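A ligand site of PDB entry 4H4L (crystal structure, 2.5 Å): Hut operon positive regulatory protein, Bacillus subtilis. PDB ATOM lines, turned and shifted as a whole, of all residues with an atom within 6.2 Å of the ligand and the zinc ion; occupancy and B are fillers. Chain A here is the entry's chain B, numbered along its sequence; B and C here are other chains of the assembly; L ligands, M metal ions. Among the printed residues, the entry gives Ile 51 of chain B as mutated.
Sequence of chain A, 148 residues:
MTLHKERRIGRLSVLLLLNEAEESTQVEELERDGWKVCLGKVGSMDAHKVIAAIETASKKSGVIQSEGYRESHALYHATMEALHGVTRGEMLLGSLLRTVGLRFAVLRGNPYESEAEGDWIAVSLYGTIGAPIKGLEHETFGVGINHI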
ATOM      1  N   ARG A  88      18.459  -9.200 -25.457  1.00  0.00           N
ATOM      2  CA  ARG A  88      18.160  -9.200 -26.861  1.00  0.00           C
ATOM      3  C   ARG A  88      19.009 -10.108 -27.746  1.00  0.00           C
ATOM      4  O   ARG A  88      19.402  -9.719 -28.836  1.00  0.00           O
ATOM      5  CB  ARG A  88      18.209  -7.750 -27.405  1.00  0.00           C
ATOM      6  CG  ARG A  88      16.975  -6.918 -27.032  1.00  0.00           C
ATOM      7  CD  ARG A  88      17.325  -5.487 -26.684  1.00  0.00           C
ATOM      8  NE  ARG A  88      18.438  -5.412 -25.723  1.00  0.00           N
ATOM      9  CZ  ARG A  88      19.636  -4.888 -25.980  1.00  0.00           C
ATOM     10  NH1 ARG A  88      19.913  -4.397 -27.184  1.00  0.00           N
ATOM     11  NH2 ARG A  88      20.543  -4.861 -25.017  1.00  0.00           N
ATOM     12  N   LEU A  96      30.450 -10.033 -23.238  1.00  0.00           N
ATOM     13  CA  LEU A  96      30.314  -9.267 -24.502  1.00  0.00           C
ATOM     14  C   LEU A  96      30.559  -7.800 -24.301  1.00  0.00           C
ATOM     15  O   LEU A  96      30.079  -6.999 -25.089  1.00  0.00           O
ATOM     16  CB  LEU A  96      28.957  -9.448 -25.173  1.00  0.00           C
ATOM     17  CG  LEU A  96      28.537 -10.830 -25.696  1.00  0.00           C
ATOM     18  CD1 LEU A  96      27.102 -10.751 -26.213  1.00  0.00           C
ATOM     19  CD2 LEU A  96      29.488 -11.362 -26.783  1.00  0.00           C
ATOM     20  N   LEU A  97      31.273  -7.439 -23.231  1.00  0.00           N
ATOM     21  CA  LEU A  97      31.758  -6.077 -23.014  1.00  0.00           C
ATOM     22  C   LEU A  97      30.643  -5.055 -22.876  1.00  0.00           C
ATOM     23  O   LEU A  97      30.697  -3.991 -23.499  1.00  0.00           O
ATOM     24  CB  LEU A  97      32.709  -5.628 -24.133  1.00  0.00           C
ATOM     25  CG  LEU A  97      33.645  -4.505 -23.675  1.00  0.00           C
ATOM     26  CD1 LEU A  97      34.815  -4.992 -22.806  1.00  0.00           C
ATOM     27  CD2 LEU A  97      34.141  -3.717 -24.893  1.00  0.00           C
ATOM     28  N   ARG A  98      29.643  -5.404 -22.075  1.00  0.00           N
ATOM     29  CA  ARG A  98      28.565  -4.483 -21.760  1.00  0.00           C
ATOM     30  C   ARG A  98      28.113  -4.699 -20.337  1.00  0.00           C
ATOM     31  O   ARG A  98      28.436  -5.727 -19.729  1.00  0.00           O
ATOM     32  CB  ARG A  98      27.387  -4.614 -22.746  1.00  0.00           C
ATOM     33  CG  ARG A  98      26.478  -5.808 -22.524  1.00  0.00           C
ATOM     34  CD  ARG A  98      25.601  -5.994 -23.743  1.00  0.00           C
ATOM     35  NE  ARG A  98      24.990  -7.309 -23.696  1.00  0.00           N
ATOM     36  CZ  ARG A  98      24.059  -7.763 -24.510  1.00  0.00           C
ATOM     37  NH1 ARG A  98      23.544  -7.003 -25.466  1.00  0.00           N
ATOM     38  NH2 ARG A  98      23.625  -9.003 -24.326  1.00  0.00           N
ATOM     39  N   THR A  99      27.381  -3.720 -19.803  1.00  0.00           N
ATOM     40  CA  THR A  99      27.033  -3.709 -18.387  1.00  0.00           C
ATOM     41  C   THR A  99      25.640  -3.113 -18.204  1.00  0.00           C
ATOM     42  O   THR A  99      25.135  -2.447 -19.110  1.00  0.00           O
ATOM     43  CB  THR A  99      28.141  -3.011 -17.527  1.00  0.00           C
ATOM     44  OG1 THR A  99      27.764  -3.033 -16.134  1.00  0.00           O
ATOM     45  CG2 THR A  99      28.372  -1.571 -17.989  1.00  0.00           C
ATOM     46  N   ILE A 129      21.800  -0.109 -20.430  1.00  0.00           N
ATOM     47  CA  ILE A 129      22.769  -1.103 -20.835  1.00  0.00           C
ATOM     48  C   ILE A 129      23.717  -0.393 -21.764  1.00  0.00           C
ATOM     49  O   ILE A 129      23.281   0.421 -22.589  1.00  0.00           O
ATOM     50  CB  ILE A 129      22.126  -2.364 -21.490  1.00  0.00           C
ATOM     51  CG1 ILE A 129      23.181  -3.469 -21.714  1.00  0.00           C
ATOM     52  CG2 ILE A 129      21.346  -2.031 -22.774  1.00  0.00           C
ATOM     53  CD1 ILE A 129      22.611  -4.684 -22.384  1.00  0.00           C
ATOM     54  N   GLY A 130      25.007  -0.647 -21.605  1.00  0.00           N
ATOM     55  CA  GLY A 130      25.978  -0.013 -22.454  1.00  0.00           C
ATOM     56  C   GLY A 130      27.352  -0.511 -22.164  1.00  0.00           C
ATOM     57  O   GLY A 130      27.528  -1.506 -21.421  1.00  0.00           O
ATOM     58  N   ALA A 131      28.323   0.224 -22.719  1.00  0.00           N
ATOM     59  CA  ALA A 131      29.763   0.012 -22.527  1.00  0.00           C
ATOM     60  C   ALA A 131      30.156   0.313 -21.085  1.00  0.00           C
ATOM     61  O   ALA A 131      29.408   1.003 -20.373  1.00  0.00           O
ATOM     62  CB  ALA A 131      30.537   0.894 -23.483  1.00  0.00           C
ATOM     63  N   PRO A 132      31.316  -0.217 -20.632  1.00  0.00           N
ATOM     64  CA  PRO A 132      31.731   0.156 -19.259  1.00  0.00           C
ATOM     65  C   PRO A 132      32.038   1.657 -19.044  1.00  0.00           C
ATOM     66  O   PRO A 132      31.874   2.145 -17.942  1.00  0.00           O
ATOM     67  CB  PRO A 132      32.957  -0.717 -18.993  1.00  0.00           C
ATOM     68  CG  PRO A 132      33.322  -1.343 -20.308  1.00  0.00           C
ATOM     69  CD  PRO A 132      32.108  -1.349 -21.163  1.00  0.00           C
ATOM     70  N   LEU A 136      27.943   5.848 -21.969  1.00  0.00           N
ATOM     71  CA  LEU A 136      27.862   5.252 -23.276  1.00  0.00           C
ATOM     72  C   LEU A 136      26.851   4.102 -23.190  1.00  0.00           C
ATOM     73  O   LEU A 136      27.255   2.947 -23.028  1.00  0.00           O
ATOM     74  CB  LEU A 136      29.247   4.770 -23.732  1.00  0.00           C
ATOM     75  CG  LEU A 136      30.406   5.762 -23.777  1.00  0.00           C
ATOM     76  CD1 LEU A 136      31.404   5.337 -24.829  1.00  0.00           C
ATOM     77  CD2 LEU A 136      29.915   7.168 -24.083  1.00  0.00           C
ATOM     78  N   GLU A 137      25.557   4.424 -23.310  1.00  0.00           N
ATOM     79  CA  GLU A 137      24.477   3.469 -23.023  1.00  0.00           C
ATOM     80  C   GLU A 137      23.127   3.920 -23.580  1.00  0.00           C
ATOM     81  O   GLU A 137      22.920   5.104 -23.855  1.00  0.00           O
ATOM     82  CB  GLU A 137      24.353   3.269 -21.506  1.00  0.00           C
ATOM     83  CG  GLU A 137      23.808   4.480 -20.767  1.00  0.00           C
ATOM     84  CD  GLU A 137      24.450   4.694 -19.415  1.00  0.00           C
ATOM     85  OE1 GLU A 137      25.665   4.439 -19.292  1.00  0.00           O
ATOM     86  OE2 GLU A 137      23.757   5.126 -18.475  1.00  0.00           O
ATOM     87  N   HIS A 138      22.222   2.954 -23.776  1.00  0.00           N
ATOM     88  CA  HIS A 138      20.816   3.255 -23.962  1.00  0.00           C
ATOM     89  C   HIS A 138      20.038   2.540 -22.906  1.00  0.00           C
ATOM     90  O   HIS A 138      20.605   1.736 -22.127  1.00  0.00           O
ATOM     91  CB  HIS A 138      20.276   2.941 -25.370  1.00  0.00           C
ATOM     92  CG  HIS A 138      20.593   1.540 -25.885  1.00  0.00           C
ATOM     93  ND1 HIS A 138      20.026   0.420 -25.364  1.00  0.00           N
ATOM     94  CD2 HIS A 138      21.362   1.112 -26.901  1.00  0.00           C
ATOM     95  CE1 HIS A 138      20.502  -0.667 -26.029  1.00  0.00           C
ATOM     96  NE2 HIS A 138      21.341  -0.236 -26.981  1.00  0.00           N
ATOM     97  N   ILE B  51      35.957  -7.559 -29.043  1.00  0.00           N
ATOM     98  CA  ILE B  51      35.190  -6.333 -29.194  1.00  0.00           C
ATOM     99  C   ILE B  51      36.054  -5.097 -28.842  1.00  0.00           C
ATOM    100  O   ILE B  51      36.036  -4.098 -29.570  1.00  0.00           O
ATOM    101  CB  ILE B  51      33.887  -6.409 -28.332  1.00  0.00           C
ATOM    102  CG1 ILE B  51      33.028  -7.585 -28.795  1.00  0.00           C
ATOM    103  CG2 ILE B  51      33.120  -5.089 -28.330  1.00  0.00           C
ATOM    104  CD1 ILE B  51      31.929  -7.958 -27.826  1.00  0.00           C
ATOM    105  N   GLU B  55      37.348  -1.869 -30.897  1.00  0.00           N
ATOM    106  CA  GLU B  55      36.827  -0.548 -30.563  1.00  0.00           C
ATOM    107  C   GLU B  55      38.013   0.399 -30.507  1.00  0.00           C
ATOM    108  O   GLU B  55      38.019   1.472 -31.153  1.00  0.00           O
ATOM    109  CB  GLU B  55      36.106  -0.562 -29.232  1.00  0.00           C
ATOM    110  CG  GLU B  55      35.307   0.691 -28.900  1.00  0.00           C
ATOM    111  CD  GLU B  55      34.780   0.715 -27.460  1.00  0.00           C
ATOM    112  OE1 GLU B  55      35.005  -0.253 -26.686  1.00  0.00           O
ATOM    113  OE2 GLU B  55      34.153   1.707 -27.069  1.00  0.00           O
ATOM    114  N   TYR B  69      28.465   8.552 -28.026  1.00  0.00           N
ATOM    115  CA  TYR B  69      27.937   7.197 -28.084  1.00  0.00           C
ATOM    116  C   TYR B  69      27.606   6.737 -29.510  1.00  0.00           C
ATOM    117  O   TYR B  69      27.993   5.648 -29.945  1.00  0.00           O
ATOM    118  CB  TYR B  69      26.691   7.111 -27.210  1.00  0.00           C
ATOM    119  CG  TYR B  69      26.198   5.700 -26.927  1.00  0.00           C
ATOM    120  CD1 TYR B  69      27.114   4.654 -26.703  1.00  0.00           C
ATOM    121  CD2 TYR B  69      24.839   5.411 -26.848  1.00  0.00           C
ATOM    122  CE1 TYR B  69      26.674   3.380 -26.429  1.00  0.00           C
ATOM    123  CE2 TYR B  69      24.395   4.131 -26.568  1.00  0.00           C
ATOM    124  CZ  TYR B  69      25.327   3.126 -26.369  1.00  0.00           C
ATOM    125  OH  TYR B  69      24.928   1.855 -26.097  1.00  0.00           O
ATOM    126  N   SER B  72      29.936   4.623 -31.507  1.00  0.00           N
ATOM    127  CA  SER B  72      30.295   3.409 -30.783  1.00  0.00           C
ATOM    128  C   SER B  72      29.188   2.395 -30.843  1.00  0.00           C
ATOM    129  O   SER B  72      29.456   1.217 -31.029  1.00  0.00           O
ATOM    130  CB  SER B  72      30.613   3.721 -29.333  1.00  0.00           C
ATOM    131  OG  SER B  72      31.836   4.384 -29.287  1.00  0.00           O
ATOM    132  N   HIS B  73      27.950   2.849 -30.678  1.00  0.00           N
ATOM    133  CA  HIS B  73      26.802   1.963 -30.789  1.00  0.00           C
ATOM    134  C   HIS B  73      26.712   1.242 -32.126  1.00  0.00           C
ATOM    135  O   HIS B  73      26.314   0.087 -32.185  1.00  0.00           O
ATOM    136  CB  HIS B  73      25.533   2.725 -30.518  1.00  0.00           C
ATOM    137  CG  HIS B  73      24.323   1.844 -30.402  1.00  0.00           C
ATOM    138  ND1 HIS B  73      23.605   1.476 -31.466  1.00  0.00           N
ATOM    139  CD2 HIS B  73      23.702   1.286 -29.294  1.00  0.00           C
ATOM    140  CE1 HIS B  73      22.576   0.721 -31.071  1.00  0.00           C
ATOM    141  NE2 HIS B  73      22.635   0.598 -29.736  1.00  0.00           N
ATOM    142  N   TYR B  76      29.620  -1.168 -32.016  1.00  0.00           N
ATOM    143  CA  TYR B  76      29.387  -2.233 -31.090  1.00  0.00           C
ATOM    144  C   TYR B  76      28.555  -3.257 -31.827  1.00  0.00           C
ATOM    145  O   TYR B  76      28.946  -4.431 -31.973  1.00  0.00           O
ATOM    146  CB  TYR B  76      28.690  -1.783 -29.837  1.00  0.00           C
ATOM    147  CG  TYR B  76      28.458  -2.940 -28.896  1.00  0.00           C
ATOM    148  CD1 TYR B  76      29.533  -3.519 -28.177  1.00  0.00           C
ATOM    149  CD2 TYR B  76      27.175  -3.472 -28.739  1.00  0.00           C
ATOM    150  CE1 TYR B  76      29.297  -4.615 -27.336  1.00  0.00           C
ATOM    151  CE2 TYR B  76      26.938  -4.539 -27.900  1.00  0.00           C
ATOM    152  CZ  TYR B  76      27.993  -5.102 -27.209  1.00  0.00           C
ATOM    153  OH  TYR B  76      27.713  -6.167 -26.397  1.00  0.00           O
ATOM    154  N   HIS B  77      27.451  -2.793 -32.397  1.00  0.00           N
ATOM    155  CA  HIS B  77      26.526  -3.684 -33.033  1.00  0.00           C
ATOM    156  C   HIS B  77      27.014  -4.330 -34.270  1.00  0.00           C
ATOM    157  O   HIS B  77      26.654  -5.483 -34.530  1.00  0.00           O
ATOM    158  CB  HIS B  77      25.203  -2.996 -33.244  1.00  0.00           C
ATOM    159  CG  HIS B  77      24.397  -2.893 -31.973  1.00  0.00           C
ATOM    160  ND1 HIS B  77      23.704  -3.925 -31.490  1.00  0.00           N
ATOM    161  CD2 HIS B  77      24.229  -1.858 -31.088  1.00  0.00           C
ATOM    162  CE1 HIS B  77      23.113  -3.566 -30.346  1.00  0.00           C
ATOM    163  NE2 HIS B  77      23.417  -2.290 -30.103  1.00  0.00           N
ATOM    164  N   GLU C  81      14.858  -6.280 -32.080  1.00  0.00           N
ATOM    165  CA  GLU C  81      15.298  -6.183 -30.719  1.00  0.00           C
ATOM    166  C   GLU C  81      14.118  -6.231 -29.789  1.00  0.00           C
ATOM    167  O   GLU C  81      14.140  -6.944 -28.774  1.00  0.00           O
ATOM    168  CB  GLU C  81      16.118  -4.901 -30.509  1.00  0.00           C
ATOM    169  CG  GLU C  81      17.566  -5.046 -30.975  1.00  0.00           C
ATOM    170  CD  GLU C  81      18.534  -4.134 -30.237  1.00  0.00           C
ATOM    171  OE1 GLU C  81      19.689  -4.020 -30.715  1.00  0.00           O
ATOM    172  OE2 GLU C  81      18.161  -3.550 -29.187  1.00  0.00           O
ATOM    173  N   TRP C 120      17.384   9.232 -32.189  1.00  0.00           N
ATOM    174  CA  TRP C 120      17.319   7.826 -31.773  1.00  0.00           C
ATOM    175  C   TRP C 120      15.922   7.281 -31.807  1.00  0.00           C
ATOM    176  O   TRP C 120      14.957   7.956 -31.457  1.00  0.00           O
ATOM    177  CB  TRP C 120      17.879   7.640 -30.379  1.00  0.00           C
ATOM    178  CG  TRP C 120      19.380   7.673 -30.333  1.00  0.00           C
ATOM    179  CD1 TRP C 120      20.216   8.772 -30.529  1.00  0.00           C
ATOM    180  CD2 TRP C 120      20.284   6.554 -30.050  1.00  0.00           C
ATOM    181  NE1 TRP C 120      21.531   8.418 -30.398  1.00  0.00           N
ATOM    182  CE2 TRP C 120      21.639   7.101 -30.108  1.00  0.00           C
ATOM    183  CE3 TRP C 120      20.114   5.207 -29.755  1.00  0.00           C
ATOM    184  CZ2 TRP C 120      22.755   6.316 -29.885  1.00  0.00           C
ATOM    185  CZ3 TRP C 120      21.242   4.430 -29.531  1.00  0.00           C
ATOM    186  CH2 TRP C 120      22.524   4.972 -29.595  1.00  0.00           C
ATOM    187  N   ILE C 145      15.977  -0.364 -29.041  1.00  0.00           N
ATOM    188  CA  ILE C 145      16.534   0.969 -29.153  1.00  0.00           C
ATOM    189  C   ILE C 145      17.721   0.981 -30.084  1.00  0.00           C
ATOM    190  O   ILE C 145      18.647   0.202 -29.903  1.00  0.00           O
ATOM    191  CB  ILE C 145      16.854   1.510 -27.759  1.00  0.00           C
ATOM    192  CG1 ILE C 145      15.552   2.026 -27.158  1.00  0.00           C
ATOM    193  CG2 ILE C 145      17.848   2.659 -27.840  1.00  0.00           C
ATOM    194  CD1 ILE C 145      15.538   2.171 -25.676  1.00  0.00           C
ATOM    195  N   ASN C 146      17.663   1.848 -31.100  1.00  0.00           N
ATOM    196  CA  ASN C 146      18.744   2.021 -32.075  1.00  0.00           C
ATOM    197  C   ASN C 146      18.989   3.485 -32.386  1.00  0.00           C
ATOM    198  O   ASN C 146      18.122   4.347 -32.139  1.00  0.00           O
ATOM    199  CB  ASN C 146      18.378   1.316 -33.370  1.00  0.00           C
ATOM    200  CG  ASN C 146      19.616   0.761 -34.107  1.00  0.00           C
ATOM    201  OD1 ASN C 146      20.750   0.878 -33.643  1.00  0.00           O
ATOM    202  ND2 ASN C 146      19.386   0.151 -35.252  1.00  0.00           N
HETATM  203  N1  LIG L   1      28.906  -2.559 -24.782  1.00  0.00           N
HETATM  204  C1  LIG L   1      27.719  -2.225 -25.604  1.00  0.00           C
HETATM  205  C2  LIG L   1      27.830  -0.823 -26.026  1.00  0.00           C
HETATM  206  O1  LIG L   1      28.843  -0.530 -26.617  1.00  0.00           O
HETATM  207  C3  LIG L   1      26.397  -2.435 -24.852  1.00  0.00           C
HETATM  208  C4  LIG L   1      25.182  -2.374 -25.749  1.00  0.00           C
HETATM  209  N2  LIG L   1      24.176  -3.300 -25.708  1.00  0.00           N
HETATM  210  C5  LIG L   1      24.857  -1.501 -26.762  1.00  0.00           C
HETATM  211  C6  LIG L   1      23.257  -2.995 -26.624  1.00  0.00           C
HETATM  212  N3  LIG L   1      23.686  -1.903 -27.272  1.00  0.00           N
HETATM  213  O2  LIG L   1      26.930   0.000 -25.796  1.00  0.00           O
HETATM  214 ZN    ZN M   1      22.305  -1.207 -28.613  1.00  0.00          ZN
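Residues that only touch the ligand: Arg 88 (3.7 Å), Arg 98 (3.2 Å), Ile 129 (3.9 Å), Gly 130 (3.4 Å) and Tyr 76 of chain B (3.3 Å). The nearest printed residue that does not touch the ligand is Leu 136 (4.1 Å).
Within 4 Å of the zinc ion: His 138, His 73 of chain B and His 77 of chain B.
O of Leu 97 sits at hydrogen-bond distance from N1 of the ligand. O2 of the ligand is in hydrogen-bond range of OH of Tyr 69 of chain B (2.7 Å). The backbone NH (N) of Ala 131 sits at hydrogen-bond distance from an oxygen (O2) of the ligand.
N3 of the ligand is bound to the zinc ion (2.0 Å). A ring nitrogen (NE2) of His 138 is bound to the zinc ion. NE2 of His 77 of chain B binds the zinc ion, at 2.2 Å. NE2 of His 73 of chain B is bound to the zinc ion (2.2 Å).
N of Ile 129 sits at hydrogen-bond distance from O of His 138 (2.8 Å). The side-chain hydroxyl of Tyr 76 of chain B sits at hydrogen-bond distance from the backbone carbonyl oxygen of Leu 96 (2.8 Å). The backbone carbonyl oxygen (O) of Leu 136 lies within hydrogen-bond range of the backbone NH (N) of Ala 131 (2.9 Å). O of Gly 130 is in hydrogen-bond range of N of Thr 99 (2.7 Å). NH1 of Arg 88 is in salt-bridge range of OE2 of Glu 81 of chain C.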
